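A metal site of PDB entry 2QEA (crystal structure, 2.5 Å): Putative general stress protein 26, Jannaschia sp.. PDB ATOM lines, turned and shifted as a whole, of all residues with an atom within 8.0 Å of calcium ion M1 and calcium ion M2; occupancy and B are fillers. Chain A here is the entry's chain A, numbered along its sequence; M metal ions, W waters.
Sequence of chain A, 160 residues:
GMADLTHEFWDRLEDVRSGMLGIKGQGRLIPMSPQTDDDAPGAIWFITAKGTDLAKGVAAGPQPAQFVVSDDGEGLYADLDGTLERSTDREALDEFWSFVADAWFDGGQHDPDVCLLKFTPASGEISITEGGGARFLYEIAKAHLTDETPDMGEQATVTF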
ATOM      1  N   HIS A   7     -26.854  13.681  30.088  1.00  0.00           N
ATOM      2  CA  HIS A   7     -26.281  12.370  30.459  1.00  0.00           C
ATOM      3  C   HIS A   7     -27.373  11.345  30.784  1.00  0.00           C
ATOM      4  O   HIS A   7     -27.278  10.201  30.351  1.00  0.00           O
ATOM      5  CB  HIS A   7     -25.305  12.478  31.650  1.00  0.00           C
ATOM      6  CG  HIS A   7     -23.989  13.095  31.317  1.00  0.00           C
ATOM      7  ND1 HIS A   7     -23.623  14.366  31.727  1.00  0.00           N
ATOM      8  CD2 HIS A   7     -22.934  12.618  30.607  1.00  0.00           C
ATOM      9  CE1 HIS A   7     -22.412  14.644  31.290  1.00  0.00           C
ATOM     10  NE2 HIS A   7     -21.973  13.601  30.609  1.00  0.00           N
ATOM     11  N   GLU A   8     -28.406  11.782  31.511  1.00  0.00           N
ATOM     12  CA  GLU A   8     -29.545  10.923  31.876  1.00  0.00           C
ATOM     13  C   GLU A   8     -30.411  10.515  30.667  1.00  0.00           C
ATOM     14  O   GLU A   8     -31.019   9.438  30.693  1.00  0.00           O
ATOM     15  CB  GLU A   8     -30.409  11.610  32.954  1.00  0.00           C
ATOM     16  CG  GLU A   8     -31.483  10.733  33.626  1.00  0.00           C
ATOM     17  CD  GLU A   8     -30.922   9.571  34.447  1.00  0.00           C
ATOM     18  OE1 GLU A   8     -29.700   9.500  34.691  1.00  0.00           O
ATOM     19  OE2 GLU A   8     -31.715   8.716  34.871  1.00  0.00           O
ATOM     20  N   PHE A   9     -30.478  11.374  29.648  1.00  0.00           N
ATOM     21  CA  PHE A   9     -31.183  11.057  28.401  1.00  0.00           C
ATOM     22  C   PHE A   9     -30.531   9.833  27.732  1.00  0.00           C
ATOM     23  O   PHE A   9     -31.216   8.859  27.409  1.00  0.00           O
ATOM     24  CB  PHE A   9     -31.239  12.267  27.432  1.00  0.00           C
ATOM     25  CG  PHE A   9     -31.598  11.915  26.012  1.00  0.00           C
ATOM     26  CD1 PHE A   9     -32.924  11.790  25.626  1.00  0.00           C
ATOM     27  CD2 PHE A   9     -30.590  11.691  25.072  1.00  0.00           C
ATOM     28  CE1 PHE A   9     -33.253  11.448  24.305  1.00  0.00           C
ATOM     29  CE2 PHE A   9     -30.897  11.344  23.748  1.00  0.00           C
ATOM     30  CZ  PHE A   9     -32.234  11.233  23.360  1.00  0.00           C
ATOM     31  N   TRP A  10     -29.208   9.894  27.539  1.00  0.00           N
ATOM     32  CA  TRP A  10     -28.430   8.784  26.942  1.00  0.00           C
ATOM     33  C   TRP A  10     -28.440   7.546  27.846  1.00  0.00           C
ATOM     34  O   TRP A  10     -28.397   6.418  27.353  1.00  0.00           O
ATOM     35  CB  TRP A  10     -26.976   9.182  26.663  1.00  0.00           C
ATOM     36  CG  TRP A  10     -26.832  10.259  25.641  1.00  0.00           C
ATOM     37  CD1 TRP A  10     -26.440  11.542  25.862  1.00  0.00           C
ATOM     38  CD2 TRP A  10     -27.113  10.158  24.245  1.00  0.00           C
ATOM     39  NE1 TRP A  10     -26.430  12.256  24.694  1.00  0.00           N
ATOM     40  CE2 TRP A  10     -26.842  11.430  23.672  1.00  0.00           C
ATOM     41  CE3 TRP A  10     -27.558   9.126  23.410  1.00  0.00           C
ATOM     42  CZ2 TRP A  10     -27.007  11.692  22.303  1.00  0.00           C
ATOM     43  CZ3 TRP A  10     -27.721   9.381  22.035  1.00  0.00           C
ATOM     44  CH2 TRP A  10     -27.441  10.660  21.514  1.00  0.00           C
ATOM     45  N   ASP A  11     -28.467   7.782  29.160  1.00  0.00           N
ATOM     46  CA  ASP A  11     -28.520   6.730  30.171  1.00  0.00           C
ATOM     47  C   ASP A  11     -29.778   5.877  29.981  1.00  0.00           C
ATOM     48  O   ASP A  11     -29.678   4.658  29.935  1.00  0.00           O
ATOM     49  CB  ASP A  11     -28.487   7.364  31.576  1.00  0.00           C
ATOM     50  CG  ASP A  11     -28.269   6.364  32.691  1.00  0.00           C
ATOM     51  OD1 ASP A  11     -28.103   5.155  32.456  1.00  0.00           O
ATOM     52  OD2 ASP A  11     -28.239   6.801  33.857  1.00  0.00           O
ATOM     53  N   ARG A  12     -30.936   6.524  29.856  1.00  0.00           N
ATOM     54  CA  ARG A  12     -32.221   5.817  29.716  1.00  0.00           C
ATOM     55  C   ARG A  12     -32.614   5.390  28.301  1.00  0.00           C
ATOM     56  O   ARG A  12     -33.378   4.439  28.158  1.00  0.00           O
ATOM     57  CB  ARG A  12     -33.331   6.645  30.342  1.00  0.00           C
ATOM     58  CG  ARG A  12     -33.130   6.857  31.820  1.00  0.00           C
ATOM     59  CD  ARG A  12     -34.273   7.610  32.394  1.00  0.00           C
ATOM     60  NE  ARG A  12     -34.117   7.831  33.836  1.00  0.00           N
ATOM     61  CZ  ARG A  12     -34.969   8.531  34.577  1.00  0.00           C
ATOM     62  NH1 ARG A  12     -36.077   9.061  34.054  1.00  0.00           N
ATOM     63  NH2 ARG A  12     -34.717   8.694  35.877  1.00  0.00           N
ATOM     64  N   LEU A  13     -32.095   6.078  27.272  1.00  0.00           N
ATOM     65  CA  LEU A  13     -32.423   5.779  25.867  1.00  0.00           C
ATOM     66  C   LEU A  13     -32.104   4.335  25.408  1.00  0.00           C
ATOM     67  O   LEU A  13     -32.761   3.820  24.508  1.00  0.00           O
ATOM     68  CB  LEU A  13     -31.772   6.802  24.911  1.00  0.00           C
ATOM     69  CG  LEU A  13     -32.077   6.736  23.403  1.00  0.00           C
ATOM     70  CD1 LEU A  13     -33.567   6.775  23.135  1.00  0.00           C
ATOM     71  CD2 LEU A  13     -31.372   7.869  22.684  1.00  0.00           C
ATOM     72  N   GLU A  14     -31.118   3.711  26.041  1.00  0.00           N
ATOM     73  CA  GLU A  14     -30.726   2.308  25.763  1.00  0.00           C
ATOM     74  C   GLU A  14     -31.866   1.308  25.950  1.00  0.00           C
ATOM     75  O   GLU A  14     -32.052   0.406  25.126  1.00  0.00           O
ATOM     76  CB  GLU A  14     -29.618   1.865  26.714  1.00  0.00           C
ATOM     77  CG  GLU A  14     -28.304   2.545  26.505  1.00  0.00           C
ATOM     78  CD  GLU A  14     -27.299   2.096  27.516  1.00  0.00           C
ATOM     79  OE1 GLU A  14     -27.577   2.189  28.734  1.00  0.00           O
ATOM     80  OE2 GLU A  14     -26.203   1.641  27.110  1.00  0.00           O
ATOM     81  N   ASP A  15     -32.591   1.464  27.056  1.00  0.00           N
ATOM     82  CA  ASP A  15     -33.745   0.602  27.390  1.00  0.00           C
ATOM     83  C   ASP A  15     -35.055   0.947  26.642  1.00  0.00           C
ATOM     84  O   ASP A  15     -36.049   0.243  26.802  1.00  0.00           O
ATOM     85  CB  ASP A  15     -33.988   0.596  28.913  1.00  0.00           C
ATOM     86  CG  ASP A  15     -32.862  -0.077  29.694  1.00  0.00           C
ATOM     87  OD1 ASP A  15     -31.722  -0.198  29.179  1.00  0.00           O
ATOM     88  OD2 ASP A  15     -33.112  -0.471  30.850  1.00  0.00           O
ATOM     89  N   THR A  36     -28.527   2.171  20.911  1.00  0.00           N
ATOM     90  CA  THR A  36     -27.492   3.049  21.492  1.00  0.00           C
ATOM     91  C   THR A  36     -26.687   2.340  22.578  1.00  0.00           C
ATOM     92  O   THR A  36     -27.043   1.238  23.018  1.00  0.00           O
ATOM     93  CB  THR A  36     -28.098   4.343  22.093  1.00  0.00           C
ATOM     94  OG1 THR A  36     -28.960   4.019  23.192  1.00  0.00           O
ATOM     95  CG2 THR A  36     -28.899   5.123  21.054  1.00  0.00           C
ATOM     96  N   ASP A  37     -25.596   2.978  22.966  1.00  0.00           N
ATOM     97  CA  ASP A  37     -24.712   2.507  24.032  1.00  0.00           C
ATOM     98  C   ASP A  37     -24.265   3.768  24.774  1.00  0.00           C
ATOM     99  O   ASP A  37     -23.656   4.646  24.172  1.00  0.00           O
ATOM    100  CB  ASP A  37     -23.524   1.737  23.445  1.00  0.00           C
ATOM    101  CG  ASP A  37     -22.749   0.919  24.485  1.00  0.00           C
ATOM    102  OD1 ASP A  37     -22.736   1.268  25.688  1.00  0.00           O
ATOM    103  OD2 ASP A  37     -22.132  -0.085  24.077  1.00  0.00           O
ATOM    104  N   ASP A  38     -24.560   3.851  26.082  1.00  0.00           N
ATOM    105  CA  ASP A  38     -24.201   5.030  26.905  1.00  0.00           C
ATOM    106  C   ASP A  38     -22.696   5.177  27.197  1.00  0.00           C
ATOM    107  O   ASP A  38     -22.289   6.187  27.771  1.00  0.00           O
ATOM    108  CB  ASP A  38     -25.080   5.201  28.163  1.00  0.00           C
ATOM    109  CG  ASP A  38     -24.993   4.037  29.154  1.00  0.00           C
ATOM    110  OD1 ASP A  38     -24.251   3.060  28.929  1.00  0.00           O
ATOM    111  OD2 ASP A  38     -25.712   4.116  30.165  1.00  0.00           O
ATOM    112  N   ASP A  39     -21.893   4.159  26.845  1.00  0.00           N
ATOM    113  CA  ASP A  39     -20.424   4.256  26.875  1.00  0.00           C
ATOM    114  C   ASP A  39     -19.941   5.176  25.739  1.00  0.00           C
ATOM    115  O   ASP A  39     -18.964   5.909  25.915  1.00  0.00           O
ATOM    116  CB  ASP A  39     -19.758   2.884  26.751  1.00  0.00           C
ATOM    117  CG  ASP A  39     -20.027   1.967  27.949  1.00  0.00           C
ATOM    118  OD1 ASP A  39     -20.878   2.296  28.808  1.00  0.00           O
ATOM    119  OD2 ASP A  39     -19.383   0.904  28.019  1.00  0.00           O
ATOM    120  N   GLU A  74     -39.393   3.659  31.301  1.00  0.00           N
ATOM    121  CA  GLU A  74     -38.164   4.400  31.605  1.00  0.00           C
ATOM    122  C   GLU A  74     -38.401   5.840  32.065  1.00  0.00           C
ATOM    123  O   GLU A  74     -37.538   6.419  32.710  1.00  0.00           O
ATOM    124  CB  GLU A  74     -37.218   4.394  30.380  1.00  0.00           C
ATOM    125  CG  GLU A  74     -36.698   3.000  30.018  1.00  0.00           C
ATOM    126  CD  GLU A  74     -35.839   2.398  31.132  1.00  0.00           C
ATOM    127  OE1 GLU A  74     -34.875   3.055  31.577  1.00  0.00           O
ATOM    128  OE2 GLU A  74     -36.123   1.247  31.541  1.00  0.00           O
HETATM  129 CA    CA M   1     -28.058   3.165  30.888  1.00  0.00          CA
HETATM  130 CA    CA M   2     -25.205   0.443  29.237  1.00  0.00          CA
HETATM  131  O   HOH W   1     -29.680   1.018  31.079  1.00  0.00           O
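Three residues have an atom within 4 Å of calcium ion M1: Asp 11, Glu 14 and Asp 38. The nearest printed residue that does not touch calcium ion M1 is Arg 12 (4.5 Å).
Within 4 Å of calcium ion M2: Glu 14 and Asp 38. Along chain A the residues within 4 Å of calcium ion M2 span positions 14 to 38. The nearest printed residue that does not touch calcium ion M2 is Asp 37 (4.4 Å).
The backbone carbonyl oxygen (O) of Asp 11 binds calcium ion M1. OE1 of Glu 14 binds calcium ion M1. OD1 of Asp 11 binds calcium ion M1 (2.5 Å). OD2 of Asp 38 is bound to calcium ion M1. Water W1 binds calcium ion M1, 2.7 Å away. Calcium ion M1 has five donor atoms within binding distance.
Calcium ion M2 is bound by the side-chain carboxylate of Glu 14 and the side-chain carboxylate of Asp 38. Slightly farther from calcium ion M2 lies the side-chain carboxylate (OE1) of Glu 14 (3.0 Å).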
